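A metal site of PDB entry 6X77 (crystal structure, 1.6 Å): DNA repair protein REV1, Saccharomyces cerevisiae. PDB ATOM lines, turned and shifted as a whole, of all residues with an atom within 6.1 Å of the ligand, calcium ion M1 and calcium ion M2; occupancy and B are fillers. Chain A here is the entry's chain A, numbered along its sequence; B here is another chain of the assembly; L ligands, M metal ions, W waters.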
ATOM      1  N   ARG A  20       7.270  31.550  -0.690  1.00  0.00           N
ATOM      2  CA  ARG A  20       6.289  30.722   0.017  1.00  0.00           C
ATOM      3  C   ARG A  20       5.718  31.446   1.237  1.00  0.00           C
ATOM      4  O   ARG A  20       4.544  31.212   1.594  1.00  0.00           O
ATOM      5  CB  ARG A  20       6.909  29.376   0.372  1.00  0.00           C
ATOM      6  CG  ARG A  20       7.350  29.239   1.808  1.00  0.00           C
ATOM      7  CD  ARG A  20       8.786  29.752   2.087  1.00  0.00           C
ATOM      8  NE  ARG A  20       9.216  29.375   3.430  1.00  0.00           N
ATOM      9  CZ  ARG A  20      10.366  29.718   4.002  1.00  0.00           C
ATOM     10  NH1 ARG A  20      11.247  30.538   3.399  1.00  0.00           N
ATOM     11  NH2 ARG A  20      10.637  29.219   5.220  1.00  0.00           N
ATOM     12  N   LEU A  21       6.496  32.328   1.860  1.00  0.00           N
ATOM     13  CA  LEU A  21       5.960  33.075   2.994  1.00  0.00           C
ATOM     14  C   LEU A  21       4.868  34.042   2.535  1.00  0.00           C
ATOM     15  O   LEU A  21       3.832  34.168   3.201  1.00  0.00           O
ATOM     16  CB  LEU A  21       7.076  33.792   3.749  1.00  0.00           C
ATOM     17  CG  LEU A  21       8.072  32.807   4.412  1.00  0.00           C
ATOM     18  CD1 LEU A  21       9.203  33.522   5.047  1.00  0.00           C
ATOM     19  CD2 LEU A  21       7.432  31.878   5.424  1.00  0.00           C
ATOM     20  N   LEU A  24       1.827  31.741   2.023  1.00  0.00           N
ATOM     21  CA  LEU A  24       1.230  31.386   3.309  1.00  0.00           C
ATOM     22  C   LEU A  24       0.324  32.493   3.825  1.00  0.00           C
ATOM     23  O   LEU A  24      -0.819  32.241   4.162  1.00  0.00           O
ATOM     24  CB  LEU A  24       2.304  31.088   4.346  1.00  0.00           C
ATOM     25  CG  LEU A  24       2.947  29.732   4.206  1.00  0.00           C
ATOM     26  CD1 LEU A  24       4.000  29.622   5.338  1.00  0.00           C
ATOM     27  CD2 LEU A  24       2.012  28.565   4.303  1.00  0.00           C
ATOM     28  N   ASP A  58      -4.268  18.956  11.042  1.00  0.00           N
ATOM     29  CA  ASP A  58      -3.135  19.581  10.343  1.00  0.00           C
ATOM     30  C   ASP A  58      -2.411  18.575   9.462  1.00  0.00           C
ATOM     31  O   ASP A  58      -2.143  17.446   9.880  1.00  0.00           O
ATOM     32  CB  ASP A  58      -2.214  20.202  11.402  1.00  0.00           C
ATOM     33  CG  ASP A  58      -0.865  20.605  10.842  1.00  0.00           C
ATOM     34  OD1 ASP A  58      -0.767  21.752  10.355  1.00  0.00           O
ATOM     35  OD2 ASP A  58       0.042  19.738  10.844  1.00  0.00           O
ATOM     36  N   PHE A  59      -2.099  18.992   8.228  1.00  0.00           N
ATOM     37  CA  PHE A  59      -1.352  18.110   7.327  1.00  0.00           C
ATOM     38  C   PHE A  59       0.054  17.844   7.883  1.00  0.00           C
ATOM     39  O   PHE A  59       0.750  18.787   8.274  1.00  0.00           O
ATOM     40  CB  PHE A  59      -1.139  18.752   5.944  1.00  0.00           C
ATOM     41  CG  PHE A  59      -2.307  18.727   5.021  1.00  0.00           C
ATOM     42  CD1 PHE A  59      -3.324  19.629   5.163  1.00  0.00           C
ATOM     43  CD2 PHE A  59      -2.274  17.914   3.913  1.00  0.00           C
ATOM     44  CE1 PHE A  59      -4.372  19.696   4.210  1.00  0.00           C
ATOM     45  CE2 PHE A  59      -3.280  17.967   2.934  1.00  0.00           C
ATOM     46  CZ  PHE A  59      -4.343  18.851   3.118  1.00  0.00           C
ATOM     47  N   ASP A  60       0.491  16.565   7.846  1.00  0.00           N
ATOM     48  CA  ASP A  60       1.880  16.228   8.129  1.00  0.00           C
ATOM     49  C   ASP A  60       2.874  16.640   7.034  1.00  0.00           C
ATOM     50  O   ASP A  60       2.711  16.304   5.852  1.00  0.00           O
ATOM     51  CB  ASP A  60       2.047  14.694   8.255  1.00  0.00           C
ATOM     52  CG  ASP A  60       1.128  14.123   9.304  1.00  0.00           C
ATOM     53  OD1 ASP A  60       1.075  14.672  10.426  1.00  0.00           O
ATOM     54  OD2 ASP A  60       0.446  13.139   8.965  1.00  0.00           O
ATOM     55  N   CYS A  61       3.920  17.370   7.447  1.00  0.00           N
ATOM     56  CA  CYS A  61       4.932  17.965   6.576  1.00  0.00           C
ATOM     57  C   CYS A  61       4.342  18.377   5.227  1.00  0.00           C
ATOM     58  O   CYS A  61       4.689  17.834   4.168  1.00  0.00           O
ATOM     59  CB  CYS A  61       6.106  17.017   6.385  1.00  0.00           C
ATOM     60  SG  CYS A  61       5.667  15.288   5.889  1.00  0.00           S
ATOM     61  N   PHE A  62       3.457  19.372   5.275  1.00  0.00           N
ATOM     62  CA  PHE A  62       2.537  19.648   4.172  1.00  0.00           C
ATOM     63  C   PHE A  62       3.223  19.823   2.820  1.00  0.00           C
ATOM     64  O   PHE A  62       2.887  19.123   1.865  1.00  0.00           O
ATOM     65  CB  PHE A  62       1.704  20.880   4.534  1.00  0.00           C
ATOM     66  CG  PHE A  62       0.711  21.304   3.484  1.00  0.00           C
ATOM     67  CD1 PHE A  62      -0.238  20.422   2.998  1.00  0.00           C
ATOM     68  CD2 PHE A  62       0.694  22.623   3.027  1.00  0.00           C
ATOM     69  CE1 PHE A  62      -1.161  20.822   2.058  1.00  0.00           C
ATOM     70  CE2 PHE A  62      -0.267  23.045   2.099  1.00  0.00           C
ATOM     71  CZ  PHE A  62      -1.168  22.146   1.594  1.00  0.00           C
ATOM     72  N   PHE A  63       4.104  20.823   2.696  1.00  0.00           N
ATOM     73  CA  PHE A  63       4.697  21.052   1.374  1.00  0.00           C
ATOM     74  C   PHE A  63       5.463  19.808   0.926  1.00  0.00           C
ATOM     75  O   PHE A  63       5.451  19.479  -0.254  1.00  0.00           O
ATOM     76  CB  PHE A  63       5.670  22.233   1.320  1.00  0.00           C
ATOM     77  CG  PHE A  63       5.034  23.603   1.325  1.00  0.00           C
ATOM     78  CD1 PHE A  63       3.672  23.781   1.519  1.00  0.00           C
ATOM     79  CD2 PHE A  63       5.830  24.730   1.120  1.00  0.00           C
ATOM     80  CE1 PHE A  63       3.122  25.035   1.583  1.00  0.00           C
ATOM     81  CE2 PHE A  63       5.277  26.007   1.168  1.00  0.00           C
ATOM     82  CZ  PHE A  63       3.930  26.155   1.379  1.00  0.00           C
ATOM     83  N   ALA A  64       6.201  19.168   1.846  1.00  0.00           N
ATOM     84  CA  ALA A  64       6.989  17.984   1.473  1.00  0.00           C
ATOM     85  C   ALA A  64       6.073  16.885   0.950  1.00  0.00           C
ATOM     86  O   ALA A  64       6.330  16.325  -0.124  1.00  0.00           O
ATOM     87  CB  ALA A  64       7.850  17.514   2.649  1.00  0.00           C
ATOM     88  N   ASP A  95      16.002  28.364   2.373  1.00  0.00           N
ATOM     89  CA  ASP A  95      15.152  27.798   3.409  1.00  0.00           C
ATOM     90  C   ASP A  95      14.559  26.448   2.994  1.00  0.00           C
ATOM     91  O   ASP A  95      14.042  26.273   1.892  1.00  0.00           O
ATOM     92  CB  ASP A  95      14.015  28.743   3.772  1.00  0.00           C
ATOM     93  CG  ASP A  95      14.422  29.851   4.720  1.00  0.00           C
ATOM     94  OD1 ASP A  95      15.617  30.176   4.897  1.00  0.00           O
ATOM     95  OD2 ASP A  95      13.488  30.456   5.263  1.00  0.00           O
ATOM     96  N   ILE A  96      14.611  25.509   3.920  1.00  0.00           N
ATOM     97  CA  ILE A  96      13.787  24.308   3.887  1.00  0.00           C
ATOM     98  C   ILE A  96      12.387  24.705   4.365  1.00  0.00           C
ATOM     99  O   ILE A  96      12.121  24.849   5.569  1.00  0.00           O
ATOM    100  CB  ILE A  96      14.403  23.192   4.745  1.00  0.00           C
ATOM    101  CG1 ILE A  96      15.715  22.723   4.091  1.00  0.00           C
ATOM    102  CG2 ILE A  96      13.423  22.065   4.881  1.00  0.00           C
ATOM    103  CD1 ILE A  96      16.651  21.995   5.085  1.00  0.00           C
ATOM    104  N   ALA A  97      11.463  24.874   3.410  1.00  0.00           N
ATOM    105  CA  ALA A  97      10.092  25.238   3.771  1.00  0.00           C
ATOM    106  C   ALA A  97       9.416  24.123   4.545  1.00  0.00           C
ATOM    107  O   ALA A  97       8.684  24.410   5.508  1.00  0.00           O
ATOM    108  CB  ALA A  97       9.266  25.605   2.524  1.00  0.00           C
ATOM    109  N   SER A  98       9.645  22.856   4.140  1.00  0.00           N
ATOM    110  CA  SER A  98       9.079  21.660   4.766  1.00  0.00           C
ATOM    111  C   SER A  98      10.042  20.498   4.545  1.00  0.00           C
ATOM    112  O   SER A  98      10.671  20.404   3.476  1.00  0.00           O
ATOM    113  CB  SER A  98       7.678  21.323   4.223  1.00  0.00           C
ATOM    114  OG  SER A  98       7.030  20.247   4.911  1.00  0.00           O
ATOM    115  N   CYS A  99      10.138  19.629   5.546  1.00  0.00           N
ATOM    116  CA  CYS A  99      10.924  18.400   5.466  1.00  0.00           C
ATOM    117  C   CYS A  99      10.095  17.248   5.997  1.00  0.00           C
ATOM    118  O   CYS A  99       9.236  17.421   6.892  1.00  0.00           O
ATOM    119  CB  CYS A  99      12.252  18.546   6.230  1.00  0.00           C
ATOM    120  SG  CYS A  99      12.070  18.964   7.980  1.00  0.00           S
ATOM    121  N   TYR A 101       9.471  13.275   7.620  1.00  0.00           N
ATOM    122  CA  TYR A 101       9.867  12.837   8.966  1.00  0.00           C
ATOM    123  C   TYR A 101      11.131  12.005   8.926  1.00  0.00           C
ATOM    124  O   TYR A 101      11.853  12.000   9.923  1.00  0.00           O
ATOM    125  CB  TYR A 101       8.697  12.118   9.655  1.00  0.00           C
ATOM    126  CG  TYR A 101       7.740  13.141  10.216  1.00  0.00           C
ATOM    127  CD1 TYR A 101       6.951  13.941   9.378  1.00  0.00           C
ATOM    128  CD2 TYR A 101       7.660  13.369  11.576  1.00  0.00           C
ATOM    129  CE1 TYR A 101       6.126  14.922   9.910  1.00  0.00           C
ATOM    130  CE2 TYR A 101       6.832  14.328  12.102  1.00  0.00           C
ATOM    131  CZ  TYR A 101       6.062  15.107  11.280  1.00  0.00           C
ATOM    132  OH  TYR A 101       5.223  16.050  11.835  1.00  0.00           O
ATOM    133  N   ARG A 104      13.622  14.646   9.468  1.00  0.00           N
ATOM    134  CA  ARG A 104      13.584  15.106  10.851  1.00  0.00           C
ATOM    135  C   ARG A 104      14.226  14.118  11.824  1.00  0.00           C
ATOM    136  O   ARG A 104      14.639  14.525  12.917  1.00  0.00           O
ATOM    137  CB  ARG A 104      12.146  15.360  11.273  1.00  0.00           C
ATOM    138  CG  ARG A 104      11.500  16.472  10.464  1.00  0.00           C
ATOM    139  CD  ARG A 104      10.065  16.761  10.912  1.00  0.00           C
ATOM    140  NE  ARG A 104       9.394  17.578   9.892  1.00  0.00           N
ATOM    141  CZ  ARG A 104       8.255  18.229  10.065  1.00  0.00           C
ATOM    142  NH1 ARG A 104       7.618  18.192  11.234  1.00  0.00           N
ATOM    143  NH2 ARG A 104       7.768  18.940   9.042  1.00  0.00           N
ATOM    144  N   ASN A 110      12.018  22.398   9.678  1.00  0.00           N
ATOM    145  CA  ASN A 110      11.526  23.488   8.817  1.00  0.00           C
ATOM    146  C   ASN A 110      12.217  24.791   9.188  1.00  0.00           C
ATOM    147  O   ASN A 110      12.424  25.089  10.374  1.00  0.00           O
ATOM    148  CB  ASN A 110      10.014  23.671   8.972  1.00  0.00           C
ATOM    149  CG  ASN A 110       9.209  22.506   8.413  1.00  0.00           C
ATOM    150  OD1 ASN A 110       9.747  21.573   7.821  1.00  0.00           O
ATOM    151  ND2 ASN A 110       7.895  22.555   8.623  1.00  0.00           N
ATOM    152  N   GLY A 111      12.601  25.556   8.177  1.00  0.00           N
ATOM    153  CA  GLY A 111      13.276  26.826   8.358  1.00  0.00           C
ATOM    154  C   GLY A 111      14.786  26.753   8.318  1.00  0.00           C
ATOM    155  O   GLY A 111      15.439  27.790   8.136  1.00  0.00           O
ATOM    156  N   TYR A 132       8.950  23.710  -5.122  1.00  0.00           N
ATOM    157  CA  TYR A 132       7.623  24.085  -4.711  1.00  0.00           C
ATOM    158  C   TYR A 132       6.600  23.752  -5.797  1.00  0.00           C
ATOM    159  O   TYR A 132       6.867  23.897  -6.988  1.00  0.00           O
ATOM    160  CB  TYR A 132       7.579  25.576  -4.428  1.00  0.00           C
ATOM    161  CG  TYR A 132       8.436  26.055  -3.255  1.00  0.00           C
ATOM    162  CD1 TYR A 132       9.746  26.472  -3.428  1.00  0.00           C
ATOM    163  CD2 TYR A 132       7.911  26.109  -1.976  1.00  0.00           C
ATOM    164  CE1 TYR A 132      10.494  26.962  -2.365  1.00  0.00           C
ATOM    165  CE2 TYR A 132       8.688  26.537  -0.895  1.00  0.00           C
ATOM    166  CZ  TYR A 132       9.954  26.990  -1.099  1.00  0.00           C
ATOM    167  OH  TYR A 132      10.713  27.496  -0.066  1.00  0.00           O
ATOM    168  N   SER A 161      -4.467  27.892   8.870  1.00  0.00           N
ATOM    169  CA  SER A 161      -3.579  28.144   7.740  1.00  0.00           C
ATOM    170  C   SER A 161      -3.999  27.208   6.605  1.00  0.00           C
ATOM    171  O   SER A 161      -4.987  26.475   6.697  1.00  0.00           O
ATOM    172  CB  SER A 161      -2.118  27.943   8.130  1.00  0.00           C
ATOM    173  OG  SER A 161      -1.870  26.547   8.222  1.00  0.00           O
ATOM    174  N   ILE A 162      -3.260  27.316   5.506  1.00  0.00           N
ATOM    175  CA  ILE A 162      -3.449  26.522   4.313  1.00  0.00           C
ATOM    176  C   ILE A 162      -3.646  25.046   4.688  1.00  0.00           C
ATOM    177  O   ILE A 162      -4.467  24.362   4.074  1.00  0.00           O
ATOM    178  CB  ILE A 162      -2.240  26.712   3.371  1.00  0.00           C
ATOM    179  CG1 ILE A 162      -2.528  26.027   2.020  1.00  0.00           C
ATOM    180  CG2 ILE A 162      -0.908  26.295   3.990  1.00  0.00           C
ATOM    181  CD1 ILE A 162      -3.564  26.707   1.274  1.00  0.00           C
ATOM    182  N   ASP A 163      -2.924  24.545   5.692  1.00  0.00           N
ATOM    183  CA  ASP A 163      -2.961  23.113   5.984  1.00  0.00           C
ATOM    184  C   ASP A 163      -3.504  22.777   7.369  1.00  0.00           C
ATOM    185  O   ASP A 163      -3.251  21.659   7.857  1.00  0.00           O
ATOM    186  CB  ASP A 163      -1.560  22.508   5.821  1.00  0.00           C
ATOM    187  CG  ASP A 163      -0.670  22.751   7.057  1.00  0.00           C
ATOM    188  OD1 ASP A 163      -0.809  23.826   7.673  1.00  0.00           O
ATOM    189  OD2 ASP A 163       0.162  21.870   7.356  1.00  0.00           O
ATOM    190  N   GLU A 164      -4.281  23.664   7.986  1.00  0.00           N
ATOM    191  CA  GLU A 164      -4.551  23.496   9.412  1.00  0.00           C
ATOM    192  C   GLU A 164      -5.838  24.183   9.814  1.00  0.00           C
ATOM    193  O   GLU A 164      -6.074  25.342   9.438  1.00  0.00           O
ATOM    194  CB  GLU A 164      -3.386  24.048  10.220  1.00  0.00           C
ATOM    195  CG  GLU A 164      -3.447  23.878  11.695  1.00  0.00           C
ATOM    196  CD  GLU A 164      -2.182  24.379  12.388  1.00  0.00           C
ATOM    197  OE1 GLU A 164      -2.202  24.430  13.652  1.00  0.00           O
ATOM    198  OE2 GLU A 164      -1.195  24.775  11.669  1.00  0.00           O
ATOM    199  N   LYS A 218       0.730  17.650  18.341  1.00  0.00           N
ATOM    200  CA  LYS A 218       2.168  17.411  18.329  1.00  0.00           C
ATOM    201  C   LYS A 218       2.496  15.969  18.702  1.00  0.00           C
ATOM    202  O   LYS A 218       3.270  15.300  18.031  1.00  0.00           O
ATOM    203  CB  LYS A 218       2.839  18.369  19.299  1.00  0.00           C
ATOM    204  CG  LYS A 218       4.333  18.429  19.166  1.00  0.00           C
ATOM    205  CD  LYS A 218       4.632  19.211  17.947  1.00  0.00           C
ATOM    206  CE  LYS A 218       5.775  18.604  17.169  1.00  0.00           C
ATOM    207  NZ  LYS A 218       6.785  17.862  18.017  1.00  0.00           N
ATOM    208  N   LYS A 221       1.742  13.274  15.843  1.00  0.00           N
ATOM    209  CA  LYS A 221       2.491  13.243  14.597  1.00  0.00           C
ATOM    210  C   LYS A 221       3.642  12.236  14.627  1.00  0.00           C
ATOM    211  O   LYS A 221       4.234  11.996  15.684  1.00  0.00           O
ATOM    212  CB  LYS A 221       3.025  14.632  14.307  1.00  0.00           C
ATOM    213  CG  LYS A 221       1.927  15.613  13.832  1.00  0.00           C
ATOM    214  CD  LYS A 221       2.431  17.010  13.583  1.00  0.00           C
ATOM    215  CE  LYS A 221       1.321  17.840  12.919  1.00  0.00           C
ATOM    216  NZ  LYS A 221       1.152  17.452  11.477  1.00  0.00           N
ATOM    217  P    DG B  12      -0.371  29.415  13.968  1.00  0.00           P
ATOM    218  OP1  DG B  12      -1.440  30.302  14.144  1.00  0.00           O
ATOM    219  OP2  DG B  12      -0.173  28.346  14.883  1.00  0.00           O
ATOM    220  O5'  DG B  12      -0.537  28.873  12.485  1.00  0.00           O
ATOM    221  C5'  DG B  12       0.233  27.788  12.006  1.00  0.00           C
ATOM    222  C4'  DG B  12       0.872  28.140  10.672  1.00  0.00           C
ATOM    223  O4'  DG B  12       1.859  29.116  10.871  1.00  0.00           O
ATOM    224  C3'  DG B  12       1.611  26.974  10.049  1.00  0.00           C
ATOM    225  O3'  DG B  12       0.753  26.256   9.194  1.00  0.00           O
ATOM    226  C2'  DG B  12       2.747  27.641   9.298  1.00  0.00           C
ATOM    227  C1'  DG B  12       2.657  29.095   9.710  1.00  0.00           C
ATOM    228  N9   DG B  12       3.910  29.759   9.997  1.00  0.00           N
ATOM    229  C8   DG B  12       4.993  29.316  10.710  1.00  0.00           C
ATOM    230  N7   DG B  12       5.952  30.199  10.771  1.00  0.00           N
ATOM    231  C5   DG B  12       5.482  31.270  10.032  1.00  0.00           C
ATOM    232  C6   DG B  12       6.087  32.526   9.752  1.00  0.00           C
ATOM    233  O6   DG B  12       7.199  32.915  10.036  1.00  0.00           O
ATOM    234  N1   DG B  12       5.251  33.322   8.976  1.00  0.00           N
ATOM    235  C2   DG B  12       3.999  32.973   8.551  1.00  0.00           C
ATOM    236  N2   DG B  12       3.380  33.864   7.776  1.00  0.00           N
ATOM    237  N3   DG B  12       3.432  31.809   8.799  1.00  0.00           N
ATOM    238  C4   DG B  12       4.230  31.011   9.539  1.00  0.00           C
HETATM  239  N1  LIG L   1       6.233  26.633   6.246  1.00  0.00           N
HETATM  240  C1  LIG L   1       7.424  27.298   5.652  1.00  0.00           C
HETATM  241  N2  LIG L   1       8.501  27.720   6.558  1.00  0.00           N
HETATM  242  C2  LIG L   1       8.444  27.405   7.941  1.00  0.00           C
HETATM  243  C3  LIG L   1       7.280  26.701   8.523  1.00  0.00           C
HETATM  244  C4  LIG L   1       6.165  26.302   7.644  1.00  0.00           C
HETATM  245  O1  LIG L   1       7.539  27.567   4.514  1.00  0.00           O
HETATM  246  N3  LIG L   1       9.523  27.754   8.786  1.00  0.00           N
HETATM  247  C5  LIG L   1       5.129  26.182   5.377  1.00  0.00           C
HETATM  248  C6  LIG L   1       5.623  24.781   4.852  1.00  0.00           C
HETATM  249  C7  LIG L   1       4.919  23.802   5.760  1.00  0.00           C
HETATM  250  C8  LIG L   1       3.700  24.393   5.878  1.00  0.00           C
HETATM  251  O2  LIG L   1       4.040  25.958   6.033  1.00  0.00           O
HETATM  252  O3  LIG L   1       4.626  22.535   5.072  1.00  0.00           O
HETATM  253  C9  LIG L   1       2.808  24.179   7.042  1.00  0.00           C
HETATM  254  O4  LIG L   1       3.529  24.562   8.202  1.00  0.00           O
HETATM  255  P1  LIG L   1       3.520  23.580   9.483  1.00  0.00           P
HETATM  256  O5  LIG L   1       2.146  23.079   9.793  1.00  0.00           O
HETATM  257  O6  LIG L   1       4.166  24.330  10.641  1.00  0.00           O
HETATM  258  O7  LIG L   1       4.584  22.414   9.166  1.00  0.00           O
HETATM  259  P2  LIG L   1       4.626  21.095   8.256  1.00  0.00           P
HETATM  260  O8  LIG L   1       3.232  20.791   7.775  1.00  0.00           O
HETATM  261  O9  LIG L   1       5.679  21.184   7.167  1.00  0.00           O
HETATM  262  O10 LIG L   1       5.099  19.976   9.295  1.00  0.00           O
HETATM  263  P3  LIG L   1       4.303  19.391  10.617  1.00  0.00           P
HETATM  264  O11 LIG L   1       3.015  20.139  10.802  1.00  0.00           O
HETATM  265  O12 LIG L   1       4.012  17.943  10.350  1.00  0.00           O
HETATM  266  O13 LIG L   1       5.281  19.579  11.759  1.00  0.00           O
HETATM  267 CA    CA M   1       1.355  20.887   9.129  1.00  0.00          CA
HETATM  268 CA    CA M   2       0.160  24.003   9.843  1.00  0.00          CA
HETATM  269  O   HOH W   1       7.006  24.205  10.809  1.00  0.00           O
HETATM  270  O   HOH W   2       4.797  19.552  14.454  1.00  0.00           O
HETATM  271  O   HOH W   3       6.973  21.616  11.974  1.00  0.00           O
HETATM  272  O   HOH W   4      11.485  29.879   8.175  1.00  0.00           O
HETATM  273  O   HOH W   5       9.267  27.485  11.628  1.00  0.00           O
HETATM  274  O   HOH W   6       2.163  21.591  13.185  1.00  0.00           O
HETATM  275  O   HOH W   7       3.924  26.419  12.615  1.00  0.00           O
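An oxygen (O12) of the ligand sits at hydrogen-bond distance from the side-chain hydroxyl (OH) of Tyr 101, 2.7 Å away. NE of Arg 20 sits at hydrogen-bond distance from O1 of the ligand (2.7 Å). The guanidinium group (NH1) of Arg 104 is in salt-bridge range of an oxygen (O13) of the ligand. O9 of the ligand lies within hydrogen-bond range of OG of Ser 98. An oxygen (O3) of the ligand is in hydrogen-bond range of the backbone NH (N) of Phe 62, at 3.4 Å. An oxygen (O12) of the ligand lies within hydrogen-bond range of the backbone NH (N) of Cys 61 (3.0 Å). The backbone NH (N) of Phe 63 sits at hydrogen-bond distance from an oxygen (O3) of the ligand, 3.0 Å away. The side-chain amide nitrogen (ND2) of Asn 110 lies within hydrogen-bond range of an oxygen (O9) of the ligand, at 3.0 Å. The side-chain amino group (NZ) of Lys 221 lies within salt-bridge range of an oxygen (O12) of the ligand, 3.1 Å away.
O of Phe 59 sits close to NZ of Lys 221 (3.5 Å). The backbone NH of Asp 163 lies close to the side-chain hydroxyl of Ser 161 (3.4 Å). The side-chain carboxylate (OD2) of Asp 58 sits close to the side-chain amino group (NZ) of Lys 221 (2.6 Å). NH1 of Arg 20 lies within salt-bridge range of OD2 of Asp 95. The guanidinium group of Arg 104 sits at hydrogen-bond distance from the backbone carbonyl oxygen of Cys 99 (3.0 Å). The backbone NH (N) of Cys 99 is in hydrogen-bond range of the side-chain amide oxygen (OD1) of Asn 110 (3.0 Å). The side-chain amino group of Lys 221 lies within salt-bridge range of the side-chain carboxylate of Asp 60 (3.0 Å). The backbone carbonyl oxygen (O) of Ile 96 is in hydrogen-bond range of the backbone NH (N) of Gly 111 (2.7 Å).
The backbone carbonyl oxygen of Ala 97 sits close to a nitrogen (N1) of the ligand (3.4 Å). Leu 24 touches the ligand. CA of Asp 60 touches O12 of the ligand (3.5 Å). N of Gly 111 touches N3 of the ligand (3.8 Å). Hydrophobic or aromatic side chains within 4 Å of the ligand: Leu 24, Phe 62, Phe 63, Ala 97 and Tyr 101. 17 residues have an atom within 4 Å of the ligand: Arg 20, Leu 24, Asp 58, Phe 59, Asp 60, Cys 61, Phe 62, Phe 63, Ala 97, Ser 98, Tyr 101, Arg 104, Asn 110, Gly 111, Asp 163, Lys 221 and DG 12 of chain B. The nearest printed residue that does not touch the ligand is Glu 164 (4.2 Å).
Within 4 Å of calcium ion M1: Asp 58, Phe 59 and Asp 163. The nearest printed residue that does not touch calcium ion M1 is Lys 221 (4.2 Å).
Merely in contact with calcium ion M2: Ser 161 (3.6 Å). Of the 27 residues printed, 5 come within 4 Å of calcium ion M2. The nearest printed residue that does not touch calcium ion M2 is Phe 59 (5.5 Å).
Calcium ion M1 is bound by O8 of the ligand (2.3 Å), O of Phe 59 (2.3 Å), OD2 of Asp 163 (2.4 Å), O5 of the ligand (2.4 Å), OD2 of Asp 58 (2.4 Å), O11 of the ligand (2.5 Å) and OD1 of Asp 58 (2.6 Å).
Calcium ion M2 is bound by an oxygen (O5) of the ligand (2.2 Å), the side-chain carboxylate (OD1) of Asp 163 (2.4 Å), the side-chain carboxylate (OE2) of Glu 164 (2.4 Å), O3' of DG 12 of chain B (2.4 Å) and the side-chain carboxylate (OD1) of Asp 58 (2.5 Å). Calcium ion M2 has five donor atoms within binding distance.
Water W1 bridges an oxygen (O6) of the ligand (2.8 Å) and the side-chain amide nitrogen of Asn 110 (2.9 Å). Water W4 bridges N3 of the ligand (3.0 Å) and NH2 of Arg 20 (3.1 Å).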
